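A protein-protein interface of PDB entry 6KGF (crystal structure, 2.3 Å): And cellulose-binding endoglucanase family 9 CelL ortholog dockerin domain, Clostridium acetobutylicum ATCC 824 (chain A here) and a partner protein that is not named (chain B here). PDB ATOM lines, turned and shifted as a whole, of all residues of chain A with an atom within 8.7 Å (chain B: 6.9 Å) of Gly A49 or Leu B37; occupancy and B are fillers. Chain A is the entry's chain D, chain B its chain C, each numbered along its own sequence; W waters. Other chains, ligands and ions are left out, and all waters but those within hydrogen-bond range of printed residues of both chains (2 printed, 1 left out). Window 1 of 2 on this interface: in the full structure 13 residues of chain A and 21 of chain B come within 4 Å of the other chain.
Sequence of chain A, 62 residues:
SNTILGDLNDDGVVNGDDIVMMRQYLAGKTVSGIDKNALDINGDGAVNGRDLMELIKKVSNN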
ATOM      1  N   MET A  22     -10.294  -9.002  32.028  1.00  0.00           N
ATOM      2  CA  MET A  22     -11.095 -10.221  32.004  1.00  0.00           C
ATOM      3  C   MET A  22     -10.893 -11.029  33.279  1.00  0.00           C
ATOM      4  O   MET A  22     -11.859 -11.493  33.896  1.00  0.00           O
ATOM      5  CB  MET A  22     -10.733 -11.057  30.777  1.00  0.00           C
ATOM      6  CG  MET A  22     -11.485 -12.373  30.680  1.00  0.00           C
ATOM      7  SD  MET A  22     -13.241 -12.137  30.352  1.00  0.00           S
ATOM      8  CE  MET A  22     -13.213 -11.784  28.594  1.00  0.00           C
ATOM      9  N   ARG A  23      -9.635 -11.212  33.687  1.00  0.00           N
ATOM     10  CA  ARG A  23      -9.353 -11.960  34.905  1.00  0.00           C
ATOM     11  C   ARG A  23      -9.998 -11.295  36.113  1.00  0.00           C
ATOM     12  O   ARG A  23     -10.664 -11.956  36.917  1.00  0.00           O
ATOM     13  CB  ARG A  23      -7.843 -12.086  35.102  1.00  0.00           C
ATOM     14  CG  ARG A  23      -7.170 -13.055  34.155  1.00  0.00           C
ATOM     15  CD  ARG A  23      -5.658 -12.985  34.297  1.00  0.00           C
ATOM     16  NE  ARG A  23      -4.985 -13.912  33.395  1.00  0.00           N
ATOM     17  CZ  ARG A  23      -3.676 -13.915  33.162  1.00  0.00           C
ATOM     18  NH1 ARG A  23      -2.885 -13.035  33.764  1.00  0.00           N
ATOM     19  NH2 ARG A  23      -3.160 -14.799  32.321  1.00  0.00           N
ATOM     20  N   LEU A  26     -13.800 -11.730  36.023  1.00  0.00           N
ATOM     21  CA  LEU A  26     -14.233 -13.086  36.334  1.00  0.00           C
ATOM     22  C   LEU A  26     -14.147 -13.381  37.826  1.00  0.00           C
ATOM     23  O   LEU A  26     -14.903 -14.216  38.335  1.00  0.00           O
ATOM     24  CB  LEU A  26     -13.399 -14.094  35.545  1.00  0.00           C
ATOM     25  CG  LEU A  26     -13.793 -14.297  34.080  1.00  0.00           C
ATOM     26  CD1 LEU A  26     -12.777 -15.180  33.378  1.00  0.00           C
ATOM     27  CD2 LEU A  26     -15.196 -14.899  33.973  1.00  0.00           C
ATOM     28  N   LEU A  39     -17.133  -8.386  26.638  1.00  0.00           N
ATOM     29  CA  LEU A  39     -16.727  -9.535  27.440  1.00  0.00           C
ATOM     30  C   LEU A  39     -17.048 -10.858  26.754  1.00  0.00           C
ATOM     31  O   LEU A  39     -16.257 -11.803  26.833  1.00  0.00           O
ATOM     32  CB  LEU A  39     -17.398  -9.472  28.811  1.00  0.00           C
ATOM     33  CG  LEU A  39     -16.855  -8.405  29.761  1.00  0.00           C
ATOM     34  CD1 LEU A  39     -17.847  -8.116  30.875  1.00  0.00           C
ATOM     35  CD2 LEU A  39     -15.517  -8.845  30.336  1.00  0.00           C
ATOM     36  N   ILE A  41     -16.710 -12.930  24.143  1.00  0.00           N
ATOM     37  CA  ILE A  41     -15.834 -12.955  22.976  1.00  0.00           C
ATOM     38  C   ILE A  41     -16.275 -14.016  21.975  1.00  0.00           C
ATOM     39  O   ILE A  41     -16.176 -13.812  20.759  1.00  0.00           O
ATOM     40  CB  ILE A  41     -14.376 -13.167  23.426  1.00  0.00           C
ATOM     41  CG1 ILE A  41     -13.852 -11.889  24.088  1.00  0.00           C
ATOM     42  CG2 ILE A  41     -13.500 -13.587  22.245  1.00  0.00           C
ATOM     43  CD1 ILE A  41     -12.476 -12.021  24.707  1.00  0.00           C
ATOM     44  N   ASN A  42     -16.753 -15.161  22.456  1.00  0.00           N
ATOM     45  CA  ASN A  42     -17.173 -16.247  21.581  1.00  0.00           C
ATOM     46  C   ASN A  42     -18.664 -16.213  21.269  1.00  0.00           C
ATOM     47  O   ASN A  42     -19.179 -17.157  20.659  1.00  0.00           O
ATOM     48  CB  ASN A  42     -16.803 -17.599  22.198  1.00  0.00           C
ATOM     49  CG  ASN A  42     -17.402 -17.801  23.576  1.00  0.00           C
ATOM     50  OD1 ASN A  42     -18.354 -17.123  23.963  1.00  0.00           O
ATOM     51  ND2 ASN A  42     -16.843 -18.744  24.327  1.00  0.00           N
ATOM     52  N   ASP A  44     -21.528 -16.704  22.859  1.00  0.00           N
ATOM     53  CA  ASP A  44     -22.365 -17.806  23.308  1.00  0.00           C
ATOM     54  C   ASP A  44     -23.366 -17.387  24.378  1.00  0.00           C
ATOM     55  O   ASP A  44     -24.081 -18.245  24.907  1.00  0.00           O
ATOM     56  CB  ASP A  44     -21.494 -18.958  23.830  1.00  0.00           C
ATOM     57  CG  ASP A  44     -20.727 -18.596  25.088  1.00  0.00           C
ATOM     58  OD1 ASP A  44     -20.836 -17.442  25.548  1.00  0.00           O
ATOM     59  OD2 ASP A  44     -20.013 -19.472  25.619  1.00  0.00           O
ATOM     60  N   ALA A  46     -22.803 -16.016  27.419  1.00  0.00           N
ATOM     61  CA  ALA A  46     -22.302 -15.974  28.784  1.00  0.00           C
ATOM     62  C   ALA A  46     -20.888 -15.413  28.801  1.00  0.00           C
ATOM     63  O   ALA A  46     -20.184 -15.414  27.789  1.00  0.00           O
ATOM     64  CB  ALA A  46     -22.316 -17.365  29.432  1.00  0.00           C
ATOM     65  N   VAL A  47     -20.483 -14.930  29.971  1.00  0.00           N
ATOM     66  CA  VAL A  47     -19.127 -14.446  30.211  1.00  0.00           C
ATOM     67  C   VAL A  47     -18.510 -15.377  31.244  1.00  0.00           C
ATOM     68  O   VAL A  47     -18.893 -15.349  32.422  1.00  0.00           O
ATOM     69  CB  VAL A  47     -19.106 -12.990  30.695  1.00  0.00           C
ATOM     70  CG1 VAL A  47     -17.670 -12.502  30.868  1.00  0.00           C
ATOM     71  CG2 VAL A  47     -19.855 -12.099  29.719  1.00  0.00           C
ATOM     72  N   ASN A  48     -17.565 -16.205  30.811  1.00  0.00           N
ATOM     73  CA  ASN A  48     -16.960 -17.193  31.691  1.00  0.00           C
ATOM     74  C   ASN A  48     -15.528 -17.445  31.234  1.00  0.00           C
ATOM     75  O   ASN A  48     -14.998 -16.737  30.371  1.00  0.00           O
ATOM     76  CB  ASN A  48     -17.804 -18.475  31.716  1.00  0.00           C
ATOM     77  CG  ASN A  48     -17.994 -19.077  30.338  1.00  0.00           C
ATOM     78  OD1 ASN A  48     -17.194 -18.849  29.427  1.00  0.00           O
ATOM     79  ND2 ASN A  48     -19.059 -19.855  30.178  1.00  0.00           N
ATOM     80  N   GLY A  49     -14.902 -18.467  31.821  1.00  0.00           N
ATOM     81  CA  GLY A  49     -13.504 -18.761  31.556  1.00  0.00           C
ATOM     82  C   GLY A  49     -13.183 -19.048  30.103  1.00  0.00           C
ATOM     83  O   GLY A  49     -12.020 -18.930  29.704  1.00  0.00           O
ATOM     84  N   ARG A  50     -14.177 -19.434  29.303  1.00  0.00           N
ATOM     85  CA  ARG A  50     -13.913 -19.703  27.897  1.00  0.00           C
ATOM     86  C   ARG A  50     -13.745 -18.425  27.088  1.00  0.00           C
ATOM     87  O   ARG A  50     -13.138 -18.461  26.014  1.00  0.00           O
ATOM     88  CB  ARG A  50     -15.031 -20.558  27.301  1.00  0.00           C
ATOM     89  CG  ARG A  50     -14.555 -21.457  26.182  1.00  0.00           C
ATOM     90  CD  ARG A  50     -15.500 -22.620  25.941  1.00  0.00           C
ATOM     91  NE  ARG A  50     -14.784 -23.771  25.399  1.00  0.00           N
ATOM     92  CZ  ARG A  50     -15.346 -24.935  25.101  1.00  0.00           C
ATOM     93  NH1 ARG A  50     -16.647 -25.119  25.289  1.00  0.00           N
ATOM     94  NH2 ARG A  50     -14.602 -25.918  24.616  1.00  0.00           N
ATOM     95  N   ASP A  51     -14.269 -17.298  27.577  1.00  0.00           N
ATOM     96  CA  ASP A  51     -13.958 -16.014  26.958  1.00  0.00           C
ATOM     97  C   ASP A  51     -12.533 -15.589  27.284  1.00  0.00           C
ATOM     98  O   ASP A  51     -11.830 -15.037  26.428  1.00  0.00           O
ATOM     99  CB  ASP A  51     -14.961 -14.961  27.418  1.00  0.00           C
ATOM    100  CG  ASP A  51     -16.375 -15.262  26.954  1.00  0.00           C
ATOM    101  OD1 ASP A  51     -16.606 -15.292  25.727  1.00  0.00           O
ATOM    102  OD2 ASP A  51     -17.251 -15.489  27.818  1.00  0.00           O
ATOM    103  N   LEU A  52     -12.088 -15.841  28.516  1.00  0.00           N
ATOM    104  CA  LEU A  52     -10.690 -15.614  28.862  1.00  0.00           C
ATOM    105  C   LEU A  52      -9.777 -16.511  28.037  1.00  0.00           C
ATOM    106  O   LEU A  52      -8.739 -16.063  27.539  1.00  0.00           O
ATOM    107  CB  LEU A  52     -10.483 -15.858  30.357  1.00  0.00           C
ATOM    108  CG  LEU A  52      -9.049 -15.794  30.885  1.00  0.00           C
ATOM    109  CD1 LEU A  52      -8.427 -14.426  30.653  1.00  0.00           C
ATOM    110  CD2 LEU A  52      -9.028 -16.150  32.365  1.00  0.00           C
ATOM    111  N   MET A  53     -10.154 -17.782  27.878  1.00  0.00           N
ATOM    112  CA  MET A  53      -9.376 -18.697  27.048  1.00  0.00           C
ATOM    113  C   MET A  53      -9.242 -18.160  25.629  1.00  0.00           C
ATOM    114  O   MET A  53      -8.147 -18.156  25.053  1.00  0.00           O
ATOM    115  CB  MET A  53     -10.036 -20.075  27.041  1.00  0.00           C
ATOM    116  CG  MET A  53      -9.187 -21.189  26.447  1.00  0.00           C
ATOM    117  SD  MET A  53      -7.948 -21.802  27.603  1.00  0.00           S
ATOM    118  CE  MET A  53      -7.424 -23.299  26.773  1.00  0.00           C
ATOM    119  N   GLU A  54     -10.355 -17.699  25.050  1.00  0.00           N
ATOM    120  CA  GLU A  54     -10.314 -17.149  23.700  1.00  0.00           C
ATOM    121  C   GLU A  54      -9.454 -15.894  23.646  1.00  0.00           C
ATOM    122  O   GLU A  54      -8.727 -15.671  22.669  1.00  0.00           O
ATOM    123  CB  GLU A  54     -11.730 -16.836  23.216  1.00  0.00           C
ATOM    124  CG  GLU A  54     -12.625 -18.053  23.031  1.00  0.00           C
ATOM    125  CD  GLU A  54     -12.466 -18.706  21.670  1.00  0.00           C
ATOM    126  OE1 GLU A  54     -11.457 -19.415  21.462  1.00  0.00           O
ATOM    127  OE2 GLU A  54     -13.352 -18.505  20.810  1.00  0.00           O
ATOM    128  N   LEU A  55      -9.529 -15.057  24.682  1.00  0.00           N
ATOM    129  CA  LEU A  55      -8.760 -13.817  24.688  1.00  0.00           C
ATOM    130  C   LEU A  55      -7.264 -14.098  24.750  1.00  0.00           C
ATOM    131  O   LEU A  55      -6.476 -13.451  24.049  1.00  0.00           O
ATOM    132  CB  LEU A  55      -9.191 -12.945  25.864  1.00  0.00           C
ATOM    133  CG  LEU A  55      -8.501 -11.587  26.000  1.00  0.00           C
ATOM    134  CD1 LEU A  55      -8.688 -10.748  24.750  1.00  0.00           C
ATOM    135  CD2 LEU A  55      -9.033 -10.852  27.223  1.00  0.00           C
ATOM    136  N   ILE A  56      -6.850 -15.057  25.584  1.00  0.00           N
ATOM    137  CA  ILE A  56      -5.438 -15.414  25.656  1.00  0.00           C
ATOM    138  C   ILE A  56      -4.967 -15.965  24.320  1.00  0.00           C
ATOM    139  O   ILE A  56      -3.815 -15.749  23.918  1.00  0.00           O
ATOM    140  CB  ILE A  56      -5.196 -16.422  26.798  1.00  0.00           C
ATOM    141  CG1 ILE A  56      -5.592 -15.808  28.143  1.00  0.00           C
ATOM    142  CG2 ILE A  56      -3.731 -16.856  26.828  1.00  0.00           C
ATOM    143  CD1 ILE A  56      -5.583 -16.789  29.296  1.00  0.00           C
ATOM    144  N   LYS A  57      -5.837 -16.687  23.614  1.00  0.00           N
ATOM    145  CA  LYS A  57      -5.480 -17.204  22.299  1.00  0.00           C
ATOM    146  C   LYS A  57      -5.258 -16.067  21.312  1.00  0.00           C
ATOM    147  O   LYS A  57      -4.254 -16.045  20.590  1.00  0.00           O
ATOM    148  CB  LYS A  57      -6.570 -18.152  21.793  1.00  0.00           C
ATOM    149  CG  LYS A  57      -6.566 -19.524  22.458  1.00  0.00           C
ATOM    150  CD  LYS A  57      -7.812 -20.336  22.103  1.00  0.00           C
ATOM    151  CE  LYS A  57      -7.901 -20.621  20.612  1.00  0.00           C
ATOM    152  NZ  LYS A  57      -9.092 -21.447  20.266  1.00  0.00           N
ATOM    153  N   PRO B  34      -4.318 -33.353  27.889  1.00  0.00           N
ATOM    154  CA  PRO B  34      -3.911 -32.234  28.747  1.00  0.00           C
ATOM    155  C   PRO B  34      -4.986 -31.165  28.804  1.00  0.00           C
ATOM    156  O   PRO B  34      -5.436 -30.654  27.770  1.00  0.00           O
ATOM    157  CB  PRO B  34      -2.626 -31.728  28.081  1.00  0.00           C
ATOM    158  CG  PRO B  34      -2.085 -32.914  27.370  1.00  0.00           C
ATOM    159  CD  PRO B  34      -3.283 -33.687  26.892  1.00  0.00           C
ATOM    160  N   VAL B  35      -5.412 -30.831  30.017  1.00  0.00           N
ATOM    161  CA  VAL B  35      -6.507 -29.895  30.232  1.00  0.00           C
ATOM    162  C   VAL B  35      -5.944 -28.486  30.353  1.00  0.00           C
ATOM    163  O   VAL B  35      -5.092 -28.218  31.208  1.00  0.00           O
ATOM    164  CB  VAL B  35      -7.316 -30.269  31.484  1.00  0.00           C
ATOM    165  CG1 VAL B  35      -8.294 -29.157  31.839  1.00  0.00           C
ATOM    166  CG2 VAL B  35      -8.046 -31.587  31.261  1.00  0.00           C
ATOM    167  N   GLY B  36      -6.436 -27.582  29.510  1.00  0.00           N
ATOM    168  CA  GLY B  36      -6.035 -26.191  29.562  1.00  0.00           C
ATOM    169  C   GLY B  36      -7.106 -25.278  30.124  1.00  0.00           C
ATOM    170  O   GLY B  36      -6.829 -24.115  30.426  1.00  0.00           O
ATOM    171  N   LEU B  37      -8.329 -25.788  30.278  1.00  0.00           N
ATOM    172  CA  LEU B  37      -9.445 -24.967  30.733  1.00  0.00           C
ATOM    173  C   LEU B  37     -10.420 -25.802  31.549  1.00  0.00           C
ATOM    174  O   LEU B  37     -10.789 -26.907  31.139  1.00  0.00           O
ATOM    175  CB  LEU B  37     -10.179 -24.334  29.543  1.00  0.00           C
ATOM    176  CG  LEU B  37     -11.550 -23.722  29.842  1.00  0.00           C
ATOM    177  CD1 LEU B  37     -11.422 -22.550  30.794  1.00  0.00           C
ATOM    178  CD2 LEU B  37     -12.231 -23.293  28.555  1.00  0.00           C
ATOM    179  N   ILE B  38     -10.847 -25.257  32.688  1.00  0.00           N
ATOM    180  CA  ILE B  38     -11.915 -25.835  33.497  1.00  0.00           C
ATOM    181  C   ILE B  38     -12.796 -24.701  34.003  1.00  0.00           C
ATOM    182  O   ILE B  38     -12.296 -23.743  34.604  1.00  0.00           O
ATOM    183  CB  ILE B  38     -11.380 -26.652  34.690  1.00  0.00           C
ATOM    184  CG1 ILE B  38     -10.479 -27.791  34.215  1.00  0.00           C
ATOM    185  CG2 ILE B  38     -12.541 -27.210  35.514  1.00  0.00           C
ATOM    186  CD1 ILE B  38      -9.762 -28.506  35.344  1.00  0.00           C
ATOM    187  N   CYS B  39     -14.101 -24.808  33.761  1.00  0.00           N
ATOM    188  CA  CYS B  39     -15.097 -23.932  34.364  1.00  0.00           C
ATOM    189  C   CYS B  39     -16.109 -24.803  35.094  1.00  0.00           C
ATOM    190  O   CYS B  39     -16.663 -25.739  34.505  1.00  0.00           O
ATOM    191  CB  CYS B  39     -15.820 -23.071  33.324  1.00  0.00           C
ATOM    192  SG  CYS B  39     -14.760 -22.046  32.285  1.00  0.00           S
ATOM    193  N   THR B  82     -12.566 -21.186  37.898  1.00  0.00           N
ATOM    194  CA  THR B  82     -12.062 -21.138  36.531  1.00  0.00           C
ATOM    195  C   THR B  82     -10.569 -21.434  36.549  1.00  0.00           C
ATOM    196  O   THR B  82      -9.797 -20.699  37.174  1.00  0.00           O
ATOM    197  CB  THR B  82     -12.320 -19.769  35.893  1.00  0.00           C
ATOM    198  OG1 THR B  82     -13.721 -19.482  35.912  1.00  0.00           O
ATOM    199  CG2 THR B  82     -11.824 -19.743  34.455  1.00  0.00           C
ATOM    200  N   PHE B  83     -10.164 -22.507  35.872  1.00  0.00           N
ATOM    201  CA  PHE B  83      -8.755 -22.790  35.640  1.00  0.00           C
ATOM    202  C   PHE B  83      -8.429 -22.557  34.172  1.00  0.00           C
ATOM    203  O   PHE B  83      -9.154 -23.022  33.287  1.00  0.00           O
ATOM    204  CB  PHE B  83      -8.384 -24.222  36.023  1.00  0.00           C
ATOM    205  CG  PHE B  83      -7.009 -24.622  35.557  1.00  0.00           C
ATOM    206  CD1 PHE B  83      -5.881 -24.209  36.246  1.00  0.00           C
ATOM    207  CD2 PHE B  83      -6.845 -25.387  34.412  1.00  0.00           C
ATOM    208  CE1 PHE B  83      -4.613 -24.564  35.811  1.00  0.00           C
ATOM    209  CE2 PHE B  83      -5.582 -25.746  33.974  1.00  0.00           C
ATOM    210  CZ  PHE B  83      -4.465 -25.334  34.674  1.00  0.00           C
ATOM    211  N   THR B  84      -7.337 -21.840  33.920  1.00  0.00           N
ATOM    212  CA  THR B  84      -6.848 -21.611  32.570  1.00  0.00           C
ATOM    213  C   THR B  84      -5.328 -21.631  32.593  1.00  0.00           C
ATOM    214  O   THR B  84      -4.711 -21.087  33.511  1.00  0.00           O
ATOM    215  CB  THR B  84      -7.335 -20.271  32.000  1.00  0.00           C
ATOM    216  OG1 THR B  84      -6.800 -19.191  32.775  1.00  0.00           O
ATOM    217  CG2 THR B  84      -8.854 -20.199  32.015  1.00  0.00           C
ATOM    218  N   ASP B  85      -4.732 -22.271  31.592  1.00  0.00           N
ATOM    219  CA  ASP B  85      -3.284 -22.220  31.429  1.00  0.00           C
ATOM    220  C   ASP B  85      -2.932 -20.906  30.738  1.00  0.00           C
ATOM    221  O   ASP B  85      -3.229 -20.737  29.548  1.00  0.00           O
ATOM    222  CB  ASP B  85      -2.777 -23.416  30.621  1.00  0.00           C
ATOM    223  CG  ASP B  85      -1.263 -23.433  30.496  1.00  0.00           C
ATOM    224  OD1 ASP B  85      -0.613 -22.480  30.975  1.00  0.00           O
ATOM    225  OD2 ASP B  85      -0.723 -24.405  29.924  1.00  0.00           O
ATOM    226  N   ILE B 125     -17.444 -26.934  32.086  1.00  0.00           N
ATOM    227  CA  ILE B 125     -16.653 -26.858  30.865  1.00  0.00           C
ATOM    228  C   ILE B 125     -15.270 -27.427  31.140  1.00  0.00           C
ATOM    229  O   ILE B 125     -14.664 -27.142  32.179  1.00  0.00           O
ATOM    230  CB  ILE B 125     -16.548 -25.411  30.338  1.00  0.00           C
ATOM    231  CG1 ILE B 125     -17.941 -24.844  30.065  1.00  0.00           C
ATOM    232  CG2 ILE B 125     -15.693 -25.363  29.073  1.00  0.00           C
ATOM    233  CD1 ILE B 125     -17.946 -23.370  29.702  1.00  0.00           C
ATOM    234  N   VAL B 126     -14.778 -28.237  30.208  1.00  0.00           N
ATOM    235  CA  VAL B 126     -13.419 -28.763  30.245  1.00  0.00           C
ATOM    236  C   VAL B 126     -12.918 -28.822  28.810  1.00  0.00           C
ATOM    237  O   VAL B 126     -13.594 -29.373  27.936  1.00  0.00           O
ATOM    238  CB  VAL B 126     -13.343 -30.155  30.900  1.00  0.00           C
ATOM    239  CG1 VAL B 126     -11.888 -30.600  31.019  1.00  0.00           C
ATOM    240  CG2 VAL B 126     -14.017 -30.147  32.264  1.00  0.00           C
ATOM    241  N   ALA B 127     -11.741 -28.251  28.565  1.00  0.00           N
ATOM    242  CA  ALA B 127     -11.214 -28.140  27.215  1.00  0.00           C
ATOM    243  C   ALA B 127      -9.704 -28.321  27.235  1.00  0.00           C
ATOM    244  O   ALA B 127      -9.055 -28.216  28.280  1.00  0.00           O
ATOM    245  CB  ALA B 127     -11.578 -26.789  26.584  1.00  0.00           C
ATOM    246  N   ASP B 128      -9.152 -28.589  26.052  1.00  0.00           N
ATOM    247  CA  ASP B 128      -7.727 -28.836  25.893  1.00  0.00           C
ATOM    248  C   ASP B 128      -6.999 -27.508  25.668  1.00  0.00           C
ATOM    249  O   ASP B 128      -7.595 -26.431  25.744  1.00  0.00           O
ATOM    250  CB  ASP B 128      -7.489 -29.835  24.758  1.00  0.00           C
ATOM    251  CG  ASP B 128      -7.909 -29.302  23.397  1.00  0.00           C
ATOM    252  OD1 ASP B 128      -8.056 -28.072  23.239  1.00  0.00           O
ATOM    253  OD2 ASP B 128      -8.089 -30.126  22.474  1.00  0.00           O
ATOM    254  N   GLU B 129      -5.698 -27.573  25.363  1.00  0.00           N
ATOM    255  CA  GLU B 129      -4.882 -26.363  25.330  1.00  0.00           C
ATOM    256  C   GLU B 129      -5.297 -25.407  24.223  1.00  0.00           C
ATOM    257  O   GLU B 129      -4.946 -24.223  24.282  1.00  0.00           O
ATOM    258  CB  GLU B 129      -3.403 -26.715  25.167  1.00  0.00           C
ATOM    259  CG  GLU B 129      -2.753 -27.274  26.422  1.00  0.00           C
ATOM    260  CD  GLU B 129      -2.542 -26.231  27.513  1.00  0.00           C
ATOM    261  OE1 GLU B 129      -1.584 -26.383  28.297  1.00  0.00           O
ATOM    262  OE2 GLU B 129      -3.327 -25.262  27.594  1.00  0.00           O
ATOM    263  N   ASP B 131      -8.591 -24.972  23.501  1.00  0.00           N
ATOM    264  CA  ASP B 131      -9.989 -24.652  23.787  1.00  0.00           C
ATOM    265  C   ASP B 131     -10.943 -25.520  22.966  1.00  0.00           C
ATOM    266  O   ASP B 131     -11.903 -25.032  22.366  1.00  0.00           O
ATOM    267  CB  ASP B 131     -10.269 -23.165  23.547  1.00  0.00           C
ATOM    268  CG  ASP B 131     -11.632 -22.739  24.066  1.00  0.00           C
ATOM    269  OD1 ASP B 131     -12.136 -23.388  25.008  1.00  0.00           O
ATOM    270  OD2 ASP B 131     -12.205 -21.769  23.525  1.00  0.00           O
ATOM    271  N   LYS B 132     -10.675 -26.823  22.944  1.00  0.00           N
ATOM    272  CA  LYS B 132     -11.549 -27.789  22.292  1.00  0.00           C
ATOM    273  C   LYS B 132     -12.199 -28.666  23.354  1.00  0.00           C
ATOM    274  O   LYS B 132     -11.513 -29.184  24.243  1.00  0.00           O
ATOM    275  CB  LYS B 132     -10.783 -28.652  21.289  1.00  0.00           C
ATOM    276  CG  LYS B 132     -10.098 -27.861  20.183  1.00  0.00           C
ATOM    277  CD  LYS B 132     -11.091 -27.049  19.366  1.00  0.00           C
ATOM    278  CE  LYS B 132     -10.397 -26.313  18.228  1.00  0.00           C
ATOM    279  NZ  LYS B 132     -11.333 -25.416  17.503  1.00  0.00           N
ATOM    280  N   ILE B 134     -13.562 -31.162  25.896  1.00  0.00           N
ATOM    281  CA  ILE B 134     -13.336 -32.505  26.417  1.00  0.00           C
ATOM    282  C   ILE B 134     -14.611 -32.912  27.144  1.00  0.00           C
ATOM    283  O   ILE B 134     -15.148 -32.135  27.942  1.00  0.00           O
ATOM    284  CB  ILE B 134     -12.118 -32.559  27.355  1.00  0.00           C
ATOM    285  CG1 ILE B 134     -10.855 -32.096  26.621  1.00  0.00           C
ATOM    286  CG2 ILE B 134     -11.931 -33.975  27.904  1.00  0.00           C
ATOM    287  CD1 ILE B 134      -9.630 -31.950  27.518  1.00  0.00           C
HETATM  288  O   HOH W   1     -15.947 -19.604  34.444  1.00  0.00           O
HETATM  289  O   HOH W   2     -15.207 -20.558  22.768  1.00  0.00           O
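The side-chain sulfur (SG) of Cys B39 lies close to the backbone NH (N) of Gly A49. The side-chain carboxylate (OD1) of Asp B131 lies within salt-bridge range of the guanidinium group (NE) of Arg A50 (2.7 Å). The side-chain carboxylate (OD2) of Asp B131 lies close to the side-chain carboxylate (OE1) of Glu A54.
The backbone carbonyl oxygen (O) of Gly B36 is in hydrogen-bond range of the backbone NH (N) of Asp B85 (3.0 Å). The backbone carbonyl oxygen of Ala B127 sits at hydrogen-bond distance from the backbone NH of Gly B36, at 3.0 Å. The side-chain carboxylate (OD2) of Asp B85 lies close to the side-chain carboxylate (OE1) of Glu B129, at 2.7 Å. The backbone NH of Lys B132 is in hydrogen-bond range of the side-chain carboxylate of Asp B128 (2.9 Å). OD2 of Asp A51 lies close to N of Asn A48, 3.1 Å away. The side-chain amino group of Lys A57 is in salt-bridge range of the side-chain carboxylate of Glu A54.
Among the printed residues, merely in contact across the chains: Asn A48 with Ile B125, Gly A49 with Leu B37, Gly A49 with Thr B82, Arg A50 with Leu B37, Arg A50 with Ile B125, Arg A50 with Ala B127, Arg A50 with Lys B132, Leu A52 with Thr B84, Met A53 with Gly B36, Met A53 with Leu B37, Met A53 with Asp B128, Met A53 with Glu B129, Met A53 with Asp B131 and Lys A57 with Asp B131.
Gly A49 touches just these residues of chain B: Leu B37, Cys B39 and Thr B82. Of chain A, only Gly A49, Arg A50 and Met A53 come within 4 Å of Leu B37. Of chain A, only Arg A50 (3.7 Å) comes within 4 Å of Ala B127. Of the printed residues of chain A, Cys B39 touches Gly A49 (3.6 Å). Printed residues of chain B within 4 Å of Glu A54: Asp B131 (3.2 Å). Printed residues of chain A within 4 Å of Asp B131: Arg A50 (2.7 Å), Met A53 (3.7 Å), Glu A54 (3.2 Å) and Lys A57 (3.9 Å). Of the printed residues of chain A, Ile B125 touches Asn A48 and Arg A50. Leu A55 touches none of the printed residues of chain B. Asp B85 touches none of the printed residues of chain A.
Of the 19 printed residues of chain A, 7 touch a printed residue of chain B. Printed residues of chain A that touch a printed residue of chain B: Asn A48, Gly A49, Arg A50, Leu A52, Met A53, Glu A54 and Lys A57. Hydrophobic or aromatic side chains of chain A that line the printed part of chain B: Leu A52 and Met A53. Hydrophobic or aromatic side chains of chain B within 4 Å of the printed part of chain A: Leu B37, Ile B125 and Ala B127. Among the printed residues, 17 pairs touch across the chains.
Water W1 lies within hydrogen-bond range of the side-chain hydroxyl (OG1) of Thr B82 (2.7 Å), the backbone NH (N) of Gly A49 (3.0 Å) and the side-chain sulfur (SG) of Cys B39 (3.5 Å). Water W2 lies within hydrogen-bond range of the side-chain amide nitrogen of Asn A42 (2.9 Å), the side-chain carboxylate of Asp B131 (3.3 Å) and the side-chain carboxylate of Glu A54 (3.4 Å).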
